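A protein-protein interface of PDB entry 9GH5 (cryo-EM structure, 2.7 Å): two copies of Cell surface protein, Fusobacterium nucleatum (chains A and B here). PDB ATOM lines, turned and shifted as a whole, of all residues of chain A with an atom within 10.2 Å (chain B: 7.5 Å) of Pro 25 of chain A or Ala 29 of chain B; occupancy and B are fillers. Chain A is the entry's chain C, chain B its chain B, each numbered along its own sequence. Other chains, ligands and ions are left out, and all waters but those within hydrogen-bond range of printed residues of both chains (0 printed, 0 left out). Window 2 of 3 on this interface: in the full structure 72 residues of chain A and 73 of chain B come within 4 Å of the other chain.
NZ of Lys 28 of chain B lies within salt-bridge range of OE1 of Glu 37 of chain B (3.7 Å). O of Ser 35 of chain B is in hydrogen-bond range of N of Gly 30 of chain B (2.7 Å). The side-chain hydroxyl of Ser 35 of chain B sits at hydrogen-bond distance from the backbone NH of Ala 32 of chain B, 3.0 Å away. The backbone NH (N) of Thr 36 of chain B is in hydrogen-bond range of the backbone carbonyl oxygen (O) of Ser 49 of chain B (3.0 Å). The backbone NH (N) of Gly 53 of chain A sits at hydrogen-bond distance from the backbone carbonyl oxygen (O) of Ala 38 of chain A (2.9 Å). The backbone carbonyl oxygen (O) of Gly 53 of chain A lies within hydrogen-bond range of the backbone NH (N) of Val 40 of chain A, at 3.4 Å.
CG1 of Ile 27 of chain B touches CB of Pro 25 of chain A (3.98 Å). Pro 25 of chain A touches Lys 28 of chain B. CD of Pro 25 of chain A touches N of Ala 29 of chain B (3.6 Å). CG of Pro 25 of chain A touches O of Ser 35 of chain B (3.8 Å). CG of Pro 25 of chain A touches OG1 of Thr 36 of chain B, at 3.5 Å. Phe 52 of chain B touches Ala 38 of chain A (CE2 to CB, 3.9 Å). Gly 39 of chain A touches Thr 36 of chain B. Phe 52 of chain A touches Phe 52 of chain B (CD2 to CE2, 3.6 Å). Phe 52 of chain B touches Gly 53 of chain A. Asp 34 of chain B touches Tyr 54 of chain A (OD2 to CE1, 3.5 Å).
Printed residues of chain B within 4 Å of Pro 25 of chain A: Ile 27 (3.98 Å), Lys 28 (3.7 Å), Ala 29 (3.6 Å), Ser 35 (3.8 Å) and Thr 36 (3.5 Å). Ile 27 of chain A touches none of the printed residues of chain B. Of the printed residues of chain B, Ala 38 of chain A touches Phe 52. Printed residues of chain B within 4 Å of Gly 39 of chain A: Thr 36 (3.9 Å). Of the printed residues of chain B, Phe 52 of chain A touches Phe 52. Printed residues of chain A within 4 Å of Ile 27 of chain B: Pro 25 (3.98 Å). Lys 28 of chain B touches just one residue of chain A: Pro 25. Ala 29 of chain B touches just one residue of chain A: Pro 25 (3.6 Å). No residue of chain A comes within 4 Å of Gly 30 of chain B. The nearest printed residue of chain B that does not touch Gly 53 of chain A is Thr 36 of chain B (4.6 Å).
Ala 38 of chain A touches Phe 52 of chain B, but with the chains exchanged Phe 52 of chain A does not touch Ala 38 of chain B (6.1 Å). Phe 52 of chain A touches its own counterpart, Phe 52 of chain B. 6 positions are printed for both chains.
Hydrophobic or aromatic side chains of chain A within 4 Å of the printed part of chain B: Pro 25, Ala 38, Phe 52 and Tyr 54. Among the printed residues, no Asp or Glu carboxylate lies within 4 Å of a Lys or Arg side-chain nitrogen of the other chain.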
ATOM      1  N   ALA A  24      -7.663  10.124   9.557  1.00  0.00           N
ATOM      2  CA  ALA A  24      -6.209  10.046   9.604  1.00  0.00           C
ATOM      3  C   ALA A  24      -5.754   8.704  10.164  1.00  0.00           C
ATOM      4  O   ALA A  24      -6.424   8.125  11.019  1.00  0.00           O
ATOM      5  CB  ALA A  24      -5.644  11.187  10.437  1.00  0.00           C
ATOM      6  N   PRO A  25      -4.621   8.205   9.671  1.00  0.00           N
ATOM      7  CA  PRO A  25      -4.085   6.943  10.192  1.00  0.00           C
ATOM      8  C   PRO A  25      -3.781   7.046  11.677  1.00  0.00           C
ATOM      9  O   PRO A  25      -3.394   8.102  12.180  1.00  0.00           O
ATOM     10  CB  PRO A  25      -2.810   6.740   9.371  1.00  0.00           C
ATOM     11  CG  PRO A  25      -3.080   7.457   8.095  1.00  0.00           C
ATOM     12  CD  PRO A  25      -3.878   8.669   8.488  1.00  0.00           C
ATOM     13  N   VAL A  26      -3.966   5.932  12.381  1.00  0.00           N
ATOM     14  CA  VAL A  26      -3.783   5.889  13.825  1.00  0.00           C
ATOM     15  C   VAL A  26      -3.121   4.572  14.206  1.00  0.00           C
ATOM     16  O   VAL A  26      -3.212   3.574  13.485  1.00  0.00           O
ATOM     17  CB  VAL A  26      -5.130   6.068  14.566  1.00  0.00           C
ATOM     18  CG1 VAL A  26      -5.949   4.789  14.509  1.00  0.00           C
ATOM     19  CG2 VAL A  26      -4.904   6.515  16.005  1.00  0.00           C
ATOM     20  N   ILE A  27      -2.436   4.583  15.347  1.00  0.00           N
ATOM     21  CA  ILE A  27      -1.884   3.385  15.966  1.00  0.00           C
ATOM     22  C   ILE A  27      -2.676   3.131  17.243  1.00  0.00           C
ATOM     23  O   ILE A  27      -2.892   4.052  18.042  1.00  0.00           O
ATOM     24  CB  ILE A  27      -0.370   3.515  16.234  1.00  0.00           C
ATOM     25  CG1 ILE A  27       0.277   2.141  16.415  1.00  0.00           C
ATOM     26  CG2 ILE A  27      -0.057   4.440  17.405  1.00  0.00           C
ATOM     27  CD1 ILE A  27       0.913   1.598  15.167  1.00  0.00           C
ATOM     28  N   LYS A  28      -3.171   1.907  17.400  1.00  0.00           N
ATOM     29  CA  LYS A  28      -4.038   1.602  18.528  1.00  0.00           C
ATOM     30  C   LYS A  28      -4.063   0.099  18.750  1.00  0.00           C
ATOM     31  O   LYS A  28      -3.662  -0.685  17.886  1.00  0.00           O
ATOM     32  CB  LYS A  28      -5.457   2.131  18.302  1.00  0.00           C
ATOM     33  CG  LYS A  28      -6.220   1.405  17.209  1.00  0.00           C
ATOM     34  CD  LYS A  28      -7.371   2.247  16.691  1.00  0.00           C
ATOM     35  CE  LYS A  28      -8.615   2.061  17.540  1.00  0.00           C
ATOM     36  NZ  LYS A  28      -8.720   0.676  18.070  1.00  0.00           N
ATOM     37  N   GLU A  37      -3.195  -2.376  15.604  1.00  0.00           N
ATOM     38  CA  GLU A  37      -3.802  -1.894  14.369  1.00  0.00           C
ATOM     39  C   GLU A  37      -3.065  -0.634  13.939  1.00  0.00           C
ATOM     40  O   GLU A  37      -3.075   0.368  14.661  1.00  0.00           O
ATOM     41  CB  GLU A  37      -5.292  -1.608  14.556  1.00  0.00           C
ATOM     42  CG  GLU A  37      -6.161  -2.846  14.622  1.00  0.00           C
ATOM     43  CD  GLU A  37      -7.572  -2.536  15.067  1.00  0.00           C
ATOM     44  OE1 GLU A  37      -7.936  -1.341  15.098  1.00  0.00           O
ATOM     45  OE2 GLU A  37      -8.319  -3.483  15.386  1.00  0.00           O
ATOM     46  N   ALA A  38      -2.432  -0.686  12.770  1.00  0.00           N
ATOM     47  CA  ALA A  38      -1.671   0.437  12.238  1.00  0.00           C
ATOM     48  C   ALA A  38      -2.226   0.798  10.872  1.00  0.00           C
ATOM     49  O   ALA A  38      -2.338  -0.066   9.997  1.00  0.00           O
ATOM     50  CB  ALA A  38      -0.183   0.102  12.139  1.00  0.00           C
ATOM     51  N   GLY A  39      -2.568   2.073  10.688  1.00  0.00           N
ATOM     52  CA  GLY A  39      -3.138   2.544   9.445  1.00  0.00           C
ATOM     53  C   GLY A  39      -4.562   3.030   9.640  1.00  0.00           C
ATOM     54  O   GLY A  39      -4.924   3.532  10.710  1.00  0.00           O
ATOM     55  N   VAL A  40      -5.365   2.866   8.595  1.00  0.00           N
ATOM     56  CA  VAL A  40      -6.753   3.307   8.588  1.00  0.00           C
ATOM     57  C   VAL A  40      -7.647   2.113   8.275  1.00  0.00           C
ATOM     58  O   VAL A  40      -7.346   1.323   7.372  1.00  0.00           O
ATOM     59  CB  VAL A  40      -6.974   4.460   7.589  1.00  0.00           C
ATOM     60  CG1 VAL A  40      -6.619   4.038   6.176  1.00  0.00           C
ATOM     61  CG2 VAL A  40      -8.409   4.954   7.656  1.00  0.00           C
ATOM     62  N   ASP A  41      -8.720   1.966   9.054  1.00  0.00           N
ATOM     63  CA  ASP A  41      -9.734   0.930   8.852  1.00  0.00           C
ATOM     64  C   ASP A  41      -9.128  -0.471   8.952  1.00  0.00           C
ATOM     65  O   ASP A  41      -9.238  -1.291   8.041  1.00  0.00           O
ATOM     66  CB  ASP A  41     -10.449   1.124   7.510  1.00  0.00           C
ATOM     67  CG  ASP A  41     -11.301   2.376   7.479  1.00  0.00           C
ATOM     68  OD1 ASP A  41     -11.126   3.238   8.365  1.00  0.00           O
ATOM     69  OD2 ASP A  41     -12.142   2.501   6.564  1.00  0.00           O
ATOM     70  N   ASN A  42      -8.502  -0.744  10.091  1.00  0.00           N
ATOM     71  CA  ASN A  42      -7.895  -2.040  10.352  1.00  0.00           C
ATOM     72  C   ASN A  42      -8.627  -2.749  11.482  1.00  0.00           C
ATOM     73  O   ASN A  42      -9.251  -2.114  12.338  1.00  0.00           O
ATOM     74  CB  ASN A  42      -6.414  -1.899  10.707  1.00  0.00           C
ATOM     75  CG  ASN A  42      -5.542  -1.692   9.489  1.00  0.00           C
ATOM     76  OD1 ASN A  42      -4.707  -2.533   9.160  1.00  0.00           O
ATOM     77  ND2 ASN A  42      -5.729  -0.567   8.813  1.00  0.00           N
ATOM     78  N   ALA A  51      -2.356  -5.929  12.337  1.00  0.00           N
ATOM     79  CA  ALA A  51      -2.838  -5.583  11.005  1.00  0.00           C
ATOM     80  C   ALA A  51      -2.283  -4.212  10.647  1.00  0.00           C
ATOM     81  O   ALA A  51      -2.666  -3.206  11.254  1.00  0.00           O
ATOM     82  CB  ALA A  51      -4.365  -5.588  10.949  1.00  0.00           C
ATOM     83  N   PHE A  52      -1.386  -4.172   9.667  1.00  0.00           N
ATOM     84  CA  PHE A  52      -0.704  -2.950   9.265  1.00  0.00           C
ATOM     85  C   PHE A  52      -1.059  -2.631   7.821  1.00  0.00           C
ATOM     86  O   PHE A  52      -0.903  -3.481   6.938  1.00  0.00           O
ATOM     87  CB  PHE A  52       0.814  -3.092   9.412  1.00  0.00           C
ATOM     88  CG  PHE A  52       1.310  -2.949  10.825  1.00  0.00           C
ATOM     89  CD1 PHE A  52       0.792  -3.729  11.844  1.00  0.00           C
ATOM     90  CD2 PHE A  52       2.314  -2.047  11.129  1.00  0.00           C
ATOM     91  CE1 PHE A  52       1.253  -3.599  13.138  1.00  0.00           C
ATOM     92  CE2 PHE A  52       2.777  -1.914  12.422  1.00  0.00           C
ATOM     93  CZ  PHE A  52       2.246  -2.692  13.427  1.00  0.00           C
ATOM     94  N   GLY A  53      -1.525  -1.409   7.582  1.00  0.00           N
ATOM     95  CA  GLY A  53      -1.885  -0.996   6.240  1.00  0.00           C
ATOM     96  C   GLY A  53      -3.292  -0.447   6.142  1.00  0.00           C
ATOM     97  O   GLY A  53      -3.736   0.297   7.021  1.00  0.00           O
ATOM     98  N   TYR A  54      -4.004  -0.803   5.075  1.00  0.00           N
ATOM     99  CA  TYR A  54      -5.370  -0.346   4.855  1.00  0.00           C
ATOM    100  C   TYR A  54      -6.293  -1.544   4.693  1.00  0.00           C
ATOM    101  O   TYR A  54      -6.033  -2.422   3.865  1.00  0.00           O
ATOM    102  CB  TYR A  54      -5.464   0.557   3.621  1.00  0.00           C
ATOM    103  CG  TYR A  54      -6.885   0.824   3.177  1.00  0.00           C
ATOM    104  CD1 TYR A  54      -7.681   1.737   3.849  1.00  0.00           C
ATOM    105  CD2 TYR A  54      -7.428   0.164   2.083  1.00  0.00           C
ATOM    106  CE1 TYR A  54      -8.978   1.985   3.451  1.00  0.00           C
ATOM    107  CE2 TYR A  54      -8.725   0.406   1.677  1.00  0.00           C
ATOM    108  CZ  TYR A  54      -9.495   1.318   2.365  1.00  0.00           C
ATOM    109  OH  TYR A  54     -10.788   1.562   1.965  1.00  0.00           O
ATOM    110  N   ILE B  27       3.265   8.566  12.542  1.00  0.00           N
ATOM    111  CA  ILE B  27       2.173   8.033  11.737  1.00  0.00           C
ATOM    112  C   ILE B  27       1.340   9.210  11.248  1.00  0.00           C
ATOM    113  O   ILE B  27       0.978  10.095  12.032  1.00  0.00           O
ATOM    114  CB  ILE B  27       1.332   7.008  12.527  1.00  0.00           C
ATOM    115  CG1 ILE B  27       0.452   6.182  11.585  1.00  0.00           C
ATOM    116  CG2 ILE B  27       0.517   7.661  13.640  1.00  0.00           C
ATOM    117  CD1 ILE B  27       1.037   4.844  11.223  1.00  0.00           C
ATOM    118  N   LYS B  28       1.084   9.252   9.944  1.00  0.00           N
ATOM    119  CA  LYS B  28       0.406  10.399   9.359  1.00  0.00           C
ATOM    120  C   LYS B  28      -0.182  10.004   8.015  1.00  0.00           C
ATOM    121  O   LYS B  28       0.209   9.001   7.413  1.00  0.00           O
ATOM    122  CB  LYS B  28       1.358  11.588   9.195  1.00  0.00           C
ATOM    123  CG  LYS B  28       2.420  11.381   8.130  1.00  0.00           C
ATOM    124  CD  LYS B  28       3.599  12.314   8.338  1.00  0.00           C
ATOM    125  CE  LYS B  28       3.352  13.667   7.699  1.00  0.00           C
ATOM    126  NZ  LYS B  28       2.540  13.552   6.457  1.00  0.00           N
ATOM    127  N   ALA B  29      -1.130  10.814   7.555  1.00  0.00           N
ATOM    128  CA  ALA B  29      -1.746  10.603   6.256  1.00  0.00           C
ATOM    129  C   ALA B  29      -0.806  11.032   5.138  1.00  0.00           C
ATOM    130  O   ALA B  29      -0.015  11.967   5.285  1.00  0.00           O
ATOM    131  CB  ALA B  29      -3.060  11.373   6.151  1.00  0.00           C
ATOM    132  N   GLY B  30      -0.898  10.334   4.011  1.00  0.00           N
ATOM    133  CA  GLY B  30      -0.125  10.698   2.842  1.00  0.00           C
ATOM    134  C   GLY B  30      -0.725  11.880   2.110  1.00  0.00           C
ATOM    135  O   GLY B  30      -1.386  12.724   2.721  1.00  0.00           O
ATOM    136  N   THR B  31      -0.505  11.955   0.800  1.00  0.00           N
ATOM    137  CA  THR B  31      -1.044  13.031  -0.017  1.00  0.00           C
ATOM    138  C   THR B  31      -2.349  12.657  -0.704  1.00  0.00           C
ATOM    139  O   THR B  31      -2.877  13.462  -1.478  1.00  0.00           O
ATOM    140  CB  THR B  31      -0.017  13.466  -1.067  1.00  0.00           C
ATOM    141  OG1 THR B  31       0.649  12.312  -1.591  1.00  0.00           O
ATOM    142  CG2 THR B  31       1.011  14.398  -0.446  1.00  0.00           C
ATOM    143  N   ALA B  32      -2.881  11.467  -0.444  1.00  0.00           N
ATOM    144  CA  ALA B  32      -4.118  11.004  -1.053  1.00  0.00           C
ATOM    145  C   ALA B  32      -5.042  10.463   0.028  1.00  0.00           C
ATOM    146  O   ALA B  32      -4.642  10.259   1.177  1.00  0.00           O
ATOM    147  CB  ALA B  32      -3.853   9.932  -2.116  1.00  0.00           C
ATOM    148  N   THR B  33      -6.297  10.240  -0.354  1.00  0.00           N
ATOM    149  CA  THR B  33      -7.288   9.731   0.585  1.00  0.00           C
ATOM    150  C   THR B  33      -6.910   8.336   1.064  1.00  0.00           C
ATOM    151  O   THR B  33      -6.557   7.465   0.264  1.00  0.00           O
ATOM    152  CB  THR B  33      -8.668   9.708  -0.070  1.00  0.00           C
ATOM    153  OG1 THR B  33      -8.921  10.969  -0.698  1.00  0.00           O
ATOM    154  CG2 THR B  33      -9.744   9.443   0.971  1.00  0.00           C
ATOM    155  N   ASP B  34      -6.987   8.131   2.380  1.00  0.00           N
ATOM    156  CA  ASP B  34      -6.707   6.838   3.007  1.00  0.00           C
ATOM    157  C   ASP B  34      -5.295   6.351   2.688  1.00  0.00           C
ATOM    158  O   ASP B  34      -5.057   5.157   2.503  1.00  0.00           O
ATOM    159  CB  ASP B  34      -7.746   5.792   2.602  1.00  0.00           C
ATOM    160  CG  ASP B  34      -9.122   6.095   3.158  1.00  0.00           C
ATOM    161  OD1 ASP B  34      -9.271   7.126   3.845  1.00  0.00           O
ATOM    162  OD2 ASP B  34     -10.054   5.303   2.906  1.00  0.00           O
ATOM    163  N   SER B  35      -4.348   7.282   2.633  1.00  0.00           N
ATOM    164  CA  SER B  35      -2.946   6.959   2.408  1.00  0.00           C
ATOM    165  C   SER B  35      -2.188   7.101   3.721  1.00  0.00           C
ATOM    166  O   SER B  35      -2.360   8.093   4.435  1.00  0.00           O
ATOM    167  CB  SER B  35      -2.338   7.863   1.337  1.00  0.00           C
ATOM    168  OG  SER B  35      -2.658   9.221   1.577  1.00  0.00           O
ATOM    169  N   THR B  36      -1.355   6.113   4.032  1.00  0.00           N
ATOM    170  CA  THR B  36      -0.691   6.020   5.324  1.00  0.00           C
ATOM    171  C   THR B  36       0.819   6.072   5.156  1.00  0.00           C
ATOM    172  O   THR B  36       1.378   5.431   4.260  1.00  0.00           O
ATOM    173  CB  THR B  36      -1.081   4.725   6.045  1.00  0.00           C
ATOM    174  OG1 THR B  36      -2.509   4.601   6.067  1.00  0.00           O
ATOM    175  CG2 THR B  36      -0.552   4.720   7.468  1.00  0.00           C
ATOM    176  N   GLU B  37       1.476   6.839   6.022  1.00  0.00           N
ATOM    177  CA  GLU B  37       2.929   6.873   6.113  1.00  0.00           C
ATOM    178  C   GLU B  37       3.325   6.522   7.539  1.00  0.00           C
ATOM    179  O   GLU B  37       2.968   7.240   8.478  1.00  0.00           O
ATOM    180  CB  GLU B  37       3.480   8.245   5.722  1.00  0.00           C
ATOM    181  CG  GLU B  37       3.472   8.516   4.231  1.00  0.00           C
ATOM    182  CD  GLU B  37       3.750   9.968   3.907  1.00  0.00           C
ATOM    183  OE1 GLU B  37       4.172  10.709   4.818  1.00  0.00           O
ATOM    184  OE2 GLU B  37       3.547  10.370   2.743  1.00  0.00           O
ATOM    185  N   ALA B  38       4.059   5.424   7.698  1.00  0.00           N
ATOM    186  CA  ALA B  38       4.506   4.959   9.004  1.00  0.00           C
ATOM    187  C   ALA B  38       6.018   4.833   8.982  1.00  0.00           C
ATOM    188  O   ALA B  38       6.577   4.202   8.079  1.00  0.00           O
ATOM    189  CB  ALA B  38       3.861   3.622   9.370  1.00  0.00           C
ATOM    190  N   ASN B  42       8.912   8.814   4.754  1.00  0.00           N
ATOM    191  CA  ASN B  42       8.068   8.012   3.883  1.00  0.00           C
ATOM    192  C   ASN B  42       7.206   8.912   3.009  1.00  0.00           C
ATOM    193  O   ASN B  42       6.887  10.046   3.377  1.00  0.00           O
ATOM    194  CB  ASN B  42       7.173   7.068   4.690  1.00  0.00           C
ATOM    195  CG  ASN B  42       7.911   5.842   5.175  1.00  0.00           C
ATOM    196  OD1 ASN B  42       7.615   4.723   4.763  1.00  0.00           O
ATOM    197  ND2 ASN B  42       8.876   6.046   6.061  1.00  0.00           N
ATOM    198  N   ALA B  44       3.646   8.539   0.528  1.00  0.00           N
ATOM    199  CA  ALA B  44       2.515   7.768   0.023  1.00  0.00           C
ATOM    200  C   ALA B  44       1.624   8.711  -0.771  1.00  0.00           C
ATOM    201  O   ALA B  44       1.064   9.658  -0.211  1.00  0.00           O
ATOM    202  CB  ALA B  44       1.738   7.108   1.161  1.00  0.00           C
ATOM    203  N   SER B  49      -3.124   3.799  -0.447  1.00  0.00           N
ATOM    204  CA  SER B  49      -1.755   3.311  -0.464  1.00  0.00           C
ATOM    205  C   SER B  49      -1.133   3.459   0.918  1.00  0.00           C
ATOM    206  O   SER B  49      -1.675   4.126   1.801  1.00  0.00           O
ATOM    207  CB  SER B  49      -0.921   4.062  -1.502  1.00  0.00           C
ATOM    208  OG  SER B  49      -0.895   5.451  -1.223  1.00  0.00           O
ATOM    209  N   PHE B  52       5.342   1.802   4.824  1.00  0.00           N
ATOM    210  CA  PHE B  52       5.731   1.498   6.194  1.00  0.00           C
ATOM    211  C   PHE B  52       7.213   1.158   6.229  1.00  0.00           C
ATOM    212  O   PHE B  52       7.670   0.281   5.489  1.00  0.00           O
ATOM    213  CB  PHE B  52       4.912   0.331   6.754  1.00  0.00           C
ATOM    214  CG  PHE B  52       3.524   0.709   7.195  1.00  0.00           C
ATOM    215  CD1 PHE B  52       2.666   1.382   6.344  1.00  0.00           C
ATOM    216  CD2 PHE B  52       3.074   0.374   8.459  1.00  0.00           C
ATOM    217  CE1 PHE B  52       1.392   1.725   6.750  1.00  0.00           C
ATOM    218  CE2 PHE B  52       1.801   0.715   8.868  1.00  0.00           C
ATOM    219  CZ  PHE B  52       0.960   1.390   8.013  1.00  0.00           C
